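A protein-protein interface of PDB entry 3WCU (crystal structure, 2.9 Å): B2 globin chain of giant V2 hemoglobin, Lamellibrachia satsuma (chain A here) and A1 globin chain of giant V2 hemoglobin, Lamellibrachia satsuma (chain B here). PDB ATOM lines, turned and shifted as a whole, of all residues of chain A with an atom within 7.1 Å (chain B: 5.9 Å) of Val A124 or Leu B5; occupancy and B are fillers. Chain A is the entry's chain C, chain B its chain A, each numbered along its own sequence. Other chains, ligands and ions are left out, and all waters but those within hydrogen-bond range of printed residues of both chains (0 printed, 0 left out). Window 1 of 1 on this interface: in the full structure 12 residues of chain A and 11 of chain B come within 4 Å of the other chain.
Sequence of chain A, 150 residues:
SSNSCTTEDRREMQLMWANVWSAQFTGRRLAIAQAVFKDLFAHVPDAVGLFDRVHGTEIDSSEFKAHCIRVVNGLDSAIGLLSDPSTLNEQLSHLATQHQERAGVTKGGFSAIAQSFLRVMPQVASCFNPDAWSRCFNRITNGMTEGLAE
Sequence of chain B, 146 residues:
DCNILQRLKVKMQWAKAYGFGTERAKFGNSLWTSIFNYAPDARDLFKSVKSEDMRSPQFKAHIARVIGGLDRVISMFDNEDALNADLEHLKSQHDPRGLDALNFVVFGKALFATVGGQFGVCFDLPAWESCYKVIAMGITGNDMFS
Among the printed residues, pairs that only touch across the chains: Val A20 with Met B12 (3.6 Å), Arg A28 with Leu B8 (3.7 Å), Ala A31 with Ile B4 (3.98 Å), Ala A31 with Leu B5 (3.7 Å), Ala A31 with Leu B8 (3.4 Å), Ala A35 with Leu B5 (3.98 Å), Val A120 with Leu B5 (3.99 Å), Gln A123 with Asn B3 (3.7 Å), Gln A123 with Gln B6 (3.9 Å), Gln A123 with Lys B9 (3.0 Å), Val A124 with Leu B5 (3.9 Å), Val A124 with Lys B9 (3.6 Å), Val A124 with Met B12 (3.1 Å) and Ser A126 with Lys B9 (3.7 Å).
Of the 9 printed residues of chain B, 7 touch a printed residue of chain A. Printed residues of chain B that touch a printed residue of chain A: Asn B3, Ile B4, Leu B5, Gln B6, Leu B8, Lys B9 and Met B12. Hydrophobic or aromatic side chains of chain B that line the printed part of chain A: Ile B4, Leu B5, Leu B8 and Met B12. Of the 17 printed residues of chain A, 10 touch a printed residue of chain B. Hydrophobic or aromatic side chains of chain A that line the printed part of chain B: Val A20, Ala A31, Ala A35, Val A120 and Val A124. Among the printed residues, no Asp or Glu carboxylate lies within 4 Å of a Lys or Arg side-chain nitrogen of the other chain.
OD1 of Asn B3 sits at hydrogen-bond distance from N of Leu B5. The guanidinium group of Arg A28 lies close to the backbone carbonyl oxygen of Val A20 (3.5 Å). The backbone carbonyl oxygen of Arg A119 is in hydrogen-bond range of the side-chain amide nitrogen of Gln A123. The backbone NH (N) of Gln B6 sits at hydrogen-bond distance from the side-chain amide oxygen (OD1) of Asn B3 (3.0 Å).
The backbone carbonyl oxygen (O) of Gln A123 sits close to the backbone carbonyl oxygen (O) of Leu B5, at 3.5 Å. The side-chain sulfur of Met B12 is in hydrogen-bond range of the guanidinium group of Arg A28 (3.0 Å). NZ of Lys B9 is in hydrogen-bond range of O of Ala A125 (3.3 Å). The side-chain amino group (NZ) of Lys B9 is in hydrogen-bond range of the backbone carbonyl oxygen (O) of Pro A122, at 3.1 Å.
Of the printed residues of chain B, Val A120 touches Leu B5. Met A121 touches none of the printed residues of chain B. Of the printed residues of chain B, Pro A122 touches Lys B9. Of chain B, only Leu B5 (3.9 Å), Lys B9 (3.6 Å) and Met B12 (3.1 Å) come within 4 Å of Val A124. Of the printed residues of chain A, Leu B5 touches Ala A31 (3.7 Å), Ala A35 (3.98 Å), Val A120 (3.99 Å), Gln A123 (3.5 Å) and Val A124 (3.9 Å). Arg B7 touches none of the printed residues of chain A. The nearest residue of chain B that does not touch Val A124 is Leu B8 (4.7 Å). The nearest printed residue of chain A that does not touch Leu B5 is Ile A32 (4.4 Å).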
ATOM      1  N   MET A  16     -36.608  -4.544 -11.628  1.00  0.00           N
ATOM      2  CA  MET A  16     -35.372  -4.029 -12.179  1.00  0.00           C
ATOM      3  C   MET A  16     -35.472  -2.526 -12.351  1.00  0.00           C
ATOM      4  O   MET A  16     -34.529  -1.801 -12.042  1.00  0.00           O
ATOM      5  CB  MET A  16     -35.081  -4.698 -13.518  1.00  0.00           C
ATOM      6  CG  MET A  16     -33.846  -4.195 -14.211  1.00  0.00           C
ATOM      7  SD  MET A  16     -34.293  -3.183 -15.616  1.00  0.00           S
ATOM      8  CE  MET A  16     -34.457  -1.611 -14.884  1.00  0.00           C
ATOM      9  N   VAL A  20     -33.439   1.286 -10.325  1.00  0.00           N
ATOM     10  CA  VAL A  20     -32.771   2.346 -11.069  1.00  0.00           C
ATOM     11  C   VAL A  20     -33.517   3.662 -11.220  1.00  0.00           C
ATOM     12  O   VAL A  20     -32.883   4.700 -11.344  1.00  0.00           O
ATOM     13  CB  VAL A  20     -32.388   1.902 -12.483  1.00  0.00           C
ATOM     14  CG1 VAL A  20     -31.089   1.151 -12.454  1.00  0.00           C
ATOM     15  CG2 VAL A  20     -33.471   1.050 -13.065  1.00  0.00           C
ATOM     16  N   ARG A  28     -29.914  10.169 -11.249  1.00  0.00           N
ATOM     17  CA  ARG A  28     -29.893   8.808 -11.725  1.00  0.00           C
ATOM     18  C   ARG A  28     -30.824   8.860 -12.932  1.00  0.00           C
ATOM     19  O   ARG A  28     -30.578   8.239 -13.969  1.00  0.00           O
ATOM     20  CB  ARG A  28     -30.446   7.859 -10.661  1.00  0.00           C
ATOM     21  CG  ARG A  28     -30.368   6.397 -11.059  1.00  0.00           C
ATOM     22  CD  ARG A  28     -28.974   5.831 -10.887  1.00  0.00           C
ATOM     23  NE  ARG A  28     -28.623   5.647  -9.474  1.00  0.00           N
ATOM     24  CZ  ARG A  28     -29.273   4.854  -8.622  1.00  0.00           C
ATOM     25  NH1 ARG A  28     -28.870   4.758  -7.362  1.00  0.00           N
ATOM     26  NH2 ARG A  28     -30.324   4.158  -9.025  1.00  0.00           N
ATOM     27  N   LEU A  30     -31.842  11.773 -14.823  1.00  0.00           N
ATOM     28  CA  LEU A  30     -31.242  12.553 -15.903  1.00  0.00           C
ATOM     29  C   LEU A  30     -30.299  11.679 -16.749  1.00  0.00           C
ATOM     30  O   LEU A  30     -30.468  11.545 -17.964  1.00  0.00           O
ATOM     31  CB  LEU A  30     -30.462  13.740 -15.324  1.00  0.00           C
ATOM     32  CG  LEU A  30     -29.897  14.723 -16.354  1.00  0.00           C
ATOM     33  CD1 LEU A  30     -31.060  15.464 -16.999  1.00  0.00           C
ATOM     34  CD2 LEU A  30     -28.918  15.689 -15.698  1.00  0.00           C
ATOM     35  N   ALA A  31     -29.315  11.081 -16.085  1.00  0.00           N
ATOM     36  CA  ALA A  31     -28.325  10.223 -16.738  1.00  0.00           C
ATOM     37  C   ALA A  31     -28.920   9.177 -17.689  1.00  0.00           C
ATOM     38  O   ALA A  31     -28.391   8.939 -18.782  1.00  0.00           O
ATOM     39  CB  ALA A  31     -27.475   9.539 -15.685  1.00  0.00           C
ATOM     40  N   ILE A  32     -30.012   8.548 -17.265  1.00  0.00           N
ATOM     41  CA  ILE A  32     -30.674   7.540 -18.087  1.00  0.00           C
ATOM     42  C   ILE A  32     -31.437   8.214 -19.227  1.00  0.00           C
ATOM     43  O   ILE A  32     -31.260   7.861 -20.395  1.00  0.00           O
ATOM     44  CB  ILE A  32     -31.658   6.676 -17.235  1.00  0.00           C
ATOM     45  CG1 ILE A  32     -30.872   5.707 -16.350  1.00  0.00           C
ATOM     46  CG2 ILE A  32     -32.604   5.899 -18.135  1.00  0.00           C
ATOM     47  CD1 ILE A  32     -31.737   4.710 -15.612  1.00  0.00           C
ATOM     48  N   ALA A  33     -32.276   9.191 -18.876  1.00  0.00           N
ATOM     49  CA  ALA A  33     -33.087   9.933 -19.843  1.00  0.00           C
ATOM     50  C   ALA A  33     -32.249  10.409 -21.020  1.00  0.00           C
ATOM     51  O   ALA A  33     -32.486  10.007 -22.161  1.00  0.00           O
ATOM     52  CB  ALA A  33     -33.749  11.116 -19.166  1.00  0.00           C
ATOM     53  N   ALA A  35     -29.184   9.636 -21.892  1.00  0.00           N
ATOM     54  CA  ALA A  35     -28.605   8.463 -22.547  1.00  0.00           C
ATOM     55  C   ALA A  35     -29.489   7.869 -23.630  1.00  0.00           C
ATOM     56  O   ALA A  35     -29.008   7.594 -24.727  1.00  0.00           O
ATOM     57  CB  ALA A  35     -28.265   7.394 -21.520  1.00  0.00           C
ATOM     58  N   VAL A  36     -30.772   7.678 -23.328  1.00  0.00           N
ATOM     59  CA  VAL A  36     -31.716   7.098 -24.288  1.00  0.00           C
ATOM     60  C   VAL A  36     -31.842   7.942 -25.567  1.00  0.00           C
ATOM     61  O   VAL A  36     -31.548   7.455 -26.664  1.00  0.00           O
ATOM     62  CB  VAL A  36     -33.123   6.920 -23.653  1.00  0.00           C
ATOM     63  CG1 VAL A  36     -33.976   6.000 -24.513  1.00  0.00           C
ATOM     64  CG2 VAL A  36     -32.993   6.353 -22.253  1.00  0.00           C
ATOM     65  N   ARG A 119     -30.127  -1.040 -25.483  1.00  0.00           N
ATOM     66  CA  ARG A 119     -28.667  -0.878 -25.445  1.00  0.00           C
ATOM     67  C   ARG A 119     -28.237   0.010 -24.278  1.00  0.00           C
ATOM     68  O   ARG A 119     -27.076   0.004 -23.876  1.00  0.00           O
ATOM     69  CB  ARG A 119     -28.140  -0.267 -26.753  1.00  0.00           C
ATOM     70  CG  ARG A 119     -28.080  -1.223 -27.944  1.00  0.00           C
ATOM     71  CD  ARG A 119     -27.650  -0.497 -29.226  1.00  0.00           C
ATOM     72  NE  ARG A 119     -28.472   0.691 -29.476  1.00  0.00           N
ATOM     73  CZ  ARG A 119     -29.194   0.901 -30.573  1.00  0.00           C
ATOM     74  NH1 ARG A 119     -29.907   2.012 -30.682  1.00  0.00           N
ATOM     75  NH2 ARG A 119     -29.207   0.013 -31.560  1.00  0.00           N
ATOM     76  N   VAL A 120     -29.181   0.770 -23.739  1.00  0.00           N
ATOM     77  CA  VAL A 120     -28.904   1.663 -22.622  1.00  0.00           C
ATOM     78  C   VAL A 120     -29.157   1.030 -21.254  1.00  0.00           C
ATOM     79  O   VAL A 120     -28.323   1.136 -20.361  1.00  0.00           O
ATOM     80  CB  VAL A 120     -29.751   2.956 -22.723  1.00  0.00           C
ATOM     81  CG1 VAL A 120     -29.689   3.738 -21.418  1.00  0.00           C
ATOM     82  CG2 VAL A 120     -29.243   3.810 -23.863  1.00  0.00           C
ATOM     83  N   MET A 121     -30.300   0.375 -21.079  1.00  0.00           N
ATOM     84  CA  MET A 121     -30.617  -0.220 -19.795  1.00  0.00           C
ATOM     85  C   MET A 121     -29.503  -1.069 -19.205  1.00  0.00           C
ATOM     86  O   MET A 121     -28.985  -0.768 -18.130  1.00  0.00           O
ATOM     87  CB  MET A 121     -31.905  -1.039 -19.886  1.00  0.00           C
ATOM     88  CG  MET A 121     -33.174  -0.186 -19.932  1.00  0.00           C
ATOM     89  SD  MET A 121     -33.169   1.281 -18.823  1.00  0.00           S
ATOM     90  CE  MET A 121     -33.731   0.589 -17.326  1.00  0.00           C
ATOM     91  N   PRO A 122     -29.091  -2.123 -19.915  1.00  0.00           N
ATOM     92  CA  PRO A 122     -28.032  -3.021 -19.450  1.00  0.00           C
ATOM     93  C   PRO A 122     -26.743  -2.366 -18.958  1.00  0.00           C
ATOM     94  O   PRO A 122     -25.833  -3.050 -18.489  1.00  0.00           O
ATOM     95  CB  PRO A 122     -27.788  -3.914 -20.663  1.00  0.00           C
ATOM     96  CG  PRO A 122     -28.080  -3.020 -21.794  1.00  0.00           C
ATOM     97  CD  PRO A 122     -29.352  -2.340 -21.344  1.00  0.00           C
ATOM     98  N   GLN A 123     -26.654  -1.051 -19.061  1.00  0.00           N
ATOM     99  CA  GLN A 123     -25.449  -0.377 -18.626  1.00  0.00           C
ATOM    100  C   GLN A 123     -25.616   0.224 -17.247  1.00  0.00           C
ATOM    101  O   GLN A 123     -24.644   0.389 -16.509  1.00  0.00           O
ATOM    102  CB  GLN A 123     -25.082   0.725 -19.609  1.00  0.00           C
ATOM    103  CG  GLN A 123     -25.031   0.256 -21.033  1.00  0.00           C
ATOM    104  CD  GLN A 123     -24.399   1.275 -21.949  1.00  0.00           C
ATOM    105  OE1 GLN A 123     -23.233   1.632 -21.785  1.00  0.00           O
ATOM    106  NE2 GLN A 123     -25.163   1.748 -22.922  1.00  0.00           N
ATOM    107  N   VAL A 124     -26.848   0.558 -16.896  1.00  0.00           N
ATOM    108  CA  VAL A 124     -27.095   1.156 -15.603  1.00  0.00           C
ATOM    109  C   VAL A 124     -27.858   0.214 -14.686  1.00  0.00           C
ATOM    110  O   VAL A 124     -27.589   0.153 -13.495  1.00  0.00           O
ATOM    111  CB  VAL A 124     -27.859   2.495 -15.767  1.00  0.00           C
ATOM    112  CG1 VAL A 124     -29.033   2.300 -16.701  1.00  0.00           C
ATOM    113  CG2 VAL A 124     -28.324   3.023 -14.408  1.00  0.00           C
ATOM    114  N   ALA A 125     -28.803  -0.533 -15.238  1.00  0.00           N
ATOM    115  CA  ALA A 125     -29.586  -1.456 -14.434  1.00  0.00           C
ATOM    116  C   ALA A 125     -28.926  -2.817 -14.423  1.00  0.00           C
ATOM    117  O   ALA A 125     -28.568  -3.353 -15.467  1.00  0.00           O
ATOM    118  CB  ALA A 125     -30.990  -1.565 -14.986  1.00  0.00           C
ATOM    119  N   SER A 126     -28.755  -3.374 -13.235  1.00  0.00           N
ATOM    120  CA  SER A 126     -28.139  -4.682 -13.111  1.00  0.00           C
ATOM    121  C   SER A 126     -29.236  -5.733 -13.168  1.00  0.00           C
ATOM    122  O   SER A 126     -30.353  -5.488 -12.712  1.00  0.00           O
ATOM    123  CB  SER A 126     -27.368  -4.764 -11.790  1.00  0.00           C
ATOM    124  OG  SER A 126     -27.964  -3.935 -10.805  1.00  0.00           O
ATOM    125  N   ASN B   3     -18.149   5.429 -18.702  1.00  0.00           N
ATOM    126  CA  ASN B   3     -19.083   6.548 -18.912  1.00  0.00           C
ATOM    127  C   ASN B   3     -19.947   6.696 -17.667  1.00  0.00           C
ATOM    128  O   ASN B   3     -19.998   5.785 -16.857  1.00  0.00           O
ATOM    129  CB  ASN B   3     -19.991   6.242 -20.110  1.00  0.00           C
ATOM    130  CG  ASN B   3     -20.821   4.955 -19.914  1.00  0.00           C
ATOM    131  OD1 ASN B   3     -21.667   4.862 -19.014  1.00  0.00           O
ATOM    132  ND2 ASN B   3     -20.571   3.960 -20.757  1.00  0.00           N
ATOM    133  N   ILE B   4     -20.657   7.805 -17.512  1.00  0.00           N
ATOM    134  CA  ILE B   4     -21.510   7.965 -16.331  1.00  0.00           C
ATOM    135  C   ILE B   4     -22.511   6.816 -16.040  1.00  0.00           C
ATOM    136  O   ILE B   4     -22.769   6.501 -14.874  1.00  0.00           O
ATOM    137  CB  ILE B   4     -22.289   9.287 -16.415  1.00  0.00           C
ATOM    138  CG1 ILE B   4     -23.515   9.247 -15.484  1.00  0.00           C
ATOM    139  CG2 ILE B   4     -22.648   9.563 -17.866  1.00  0.00           C
ATOM    140  CD1 ILE B   4     -23.195   9.541 -13.998  1.00  0.00           C
ATOM    141  N   LEU B   5     -23.089   6.222 -17.088  1.00  0.00           N
ATOM    142  CA  LEU B   5     -24.040   5.111 -16.948  1.00  0.00           C
ATOM    143  C   LEU B   5     -23.450   3.998 -16.073  1.00  0.00           C
ATOM    144  O   LEU B   5     -24.085   3.541 -15.125  1.00  0.00           O
ATOM    145  CB  LEU B   5     -24.419   4.540 -18.328  1.00  0.00           C
ATOM    146  CG  LEU B   5     -25.463   5.297 -19.156  1.00  0.00           C
ATOM    147  CD1 LEU B   5     -25.913   4.374 -20.287  1.00  0.00           C
ATOM    148  CD2 LEU B   5     -26.664   5.702 -18.290  1.00  0.00           C
ATOM    149  N   GLN B   6     -22.230   3.577 -16.396  1.00  0.00           N
ATOM    150  CA  GLN B   6     -21.546   2.549 -15.624  1.00  0.00           C
ATOM    151  C   GLN B   6     -21.103   3.045 -14.257  1.00  0.00           C
ATOM    152  O   GLN B   6     -20.988   2.263 -13.314  1.00  0.00           O
ATOM    153  CB  GLN B   6     -20.334   2.051 -16.383  1.00  0.00           C
ATOM    154  CG  GLN B   6     -20.701   1.222 -17.570  1.00  0.00           C
ATOM    155  CD  GLN B   6     -19.550   1.052 -18.517  1.00  0.00           C
ATOM    156  OE1 GLN B   6     -18.957   2.037 -18.958  1.00  0.00           O
ATOM    157  NE2 GLN B   6     -19.222  -0.197 -18.846  1.00  0.00           N
ATOM    158  N   ARG B   7     -20.830   4.338 -14.153  1.00  0.00           N
ATOM    159  CA  ARG B   7     -20.424   4.907 -12.877  1.00  0.00           C
ATOM    160  C   ARG B   7     -21.609   4.812 -11.908  1.00  0.00           C
ATOM    161  O   ARG B   7     -21.457   4.333 -10.784  1.00  0.00           O
ATOM    162  CB  ARG B   7     -19.955   6.357 -13.071  1.00  0.00           C
ATOM    163  CG  ARG B   7     -18.605   6.450 -13.773  1.00  0.00           C
ATOM    164  CD  ARG B   7     -18.239   7.866 -14.219  1.00  0.00           C
ATOM    165  NE  ARG B   7     -16.889   7.901 -14.784  1.00  0.00           N
ATOM    166  CZ  ARG B   7     -15.904   8.658 -14.312  1.00  0.00           C
ATOM    167  NH1 ARG B   7     -16.127   9.446 -13.274  1.00  0.00           N
ATOM    168  NH2 ARG B   7     -14.693   8.613 -14.854  1.00  0.00           N
ATOM    169  N   LEU B   8     -22.790   5.243 -12.347  1.00  0.00           N
ATOM    170  CA  LEU B   8     -23.982   5.151 -11.509  1.00  0.00           C
ATOM    171  C   LEU B   8     -24.256   3.688 -11.149  1.00  0.00           C
ATOM    172  O   LEU B   8     -24.812   3.397 -10.086  1.00  0.00           O
ATOM    173  CB  LEU B   8     -25.206   5.732 -12.226  1.00  0.00           C
ATOM    174  CG  LEU B   8     -25.232   7.256 -12.373  1.00  0.00           C
ATOM    175  CD1 LEU B   8     -26.569   7.726 -12.925  1.00  0.00           C
ATOM    176  CD2 LEU B   8     -25.014   7.881 -11.020  1.00  0.00           C
ATOM    177  N   LYS B   9     -23.862   2.775 -12.040  1.00  0.00           N
ATOM    178  CA  LYS B   9     -24.063   1.343 -11.830  1.00  0.00           C
ATOM    179  C   LYS B   9     -23.096   0.781 -10.822  1.00  0.00           C
ATOM    180  O   LYS B   9     -23.513   0.149  -9.860  1.00  0.00           O
ATOM    181  CB  LYS B   9     -23.898   0.562 -13.126  1.00  0.00           C
ATOM    182  CG  LYS B   9     -24.240  -0.908 -12.959  1.00  0.00           C
ATOM    183  CD  LYS B   9     -24.303  -1.608 -14.282  1.00  0.00           C
ATOM    184  CE  LYS B   9     -25.119  -2.853 -14.179  1.00  0.00           C
ATOM    185  NZ  LYS B   9     -25.266  -3.477 -15.513  1.00  0.00           N
ATOM    186  N   VAL B  10     -21.805   0.982 -11.056  1.00  0.00           N
ATOM    187  CA  VAL B  10     -20.801   0.496 -10.127  1.00  0.00           C
ATOM    188  C   VAL B  10     -21.111   1.033  -8.739  1.00  0.00           C
ATOM    189  O   VAL B  10     -20.810   0.386  -7.742  1.00  0.00           O
ATOM    190  CB  VAL B  10     -19.384   0.936 -10.535  1.00  0.00           C
ATOM    191  CG1 VAL B  10     -18.438   0.815  -9.348  1.00  0.00           C
ATOM    192  CG2 VAL B  10     -18.882   0.062 -11.686  1.00  0.00           C
ATOM    193  N   MET B  12     -24.165   1.530  -7.404  1.00  0.00           N
ATOM    194  CA  MET B  12     -25.221   0.705  -6.831  1.00  0.00           C
ATOM    195  C   MET B  12     -24.736  -0.687  -6.461  1.00  0.00           C
ATOM    196  O   MET B  12     -24.947  -1.140  -5.335  1.00  0.00           O
ATOM    197  CB  MET B  12     -26.403   0.595  -7.781  1.00  0.00           C
ATOM    198  CG  MET B  12     -27.119   1.900  -8.013  1.00  0.00           C
ATOM    199  SD  MET B  12     -28.635   1.629  -8.946  1.00  0.00           S
ATOM    200  CE  MET B  12     -27.967   1.355 -10.612  1.00  0.00           C
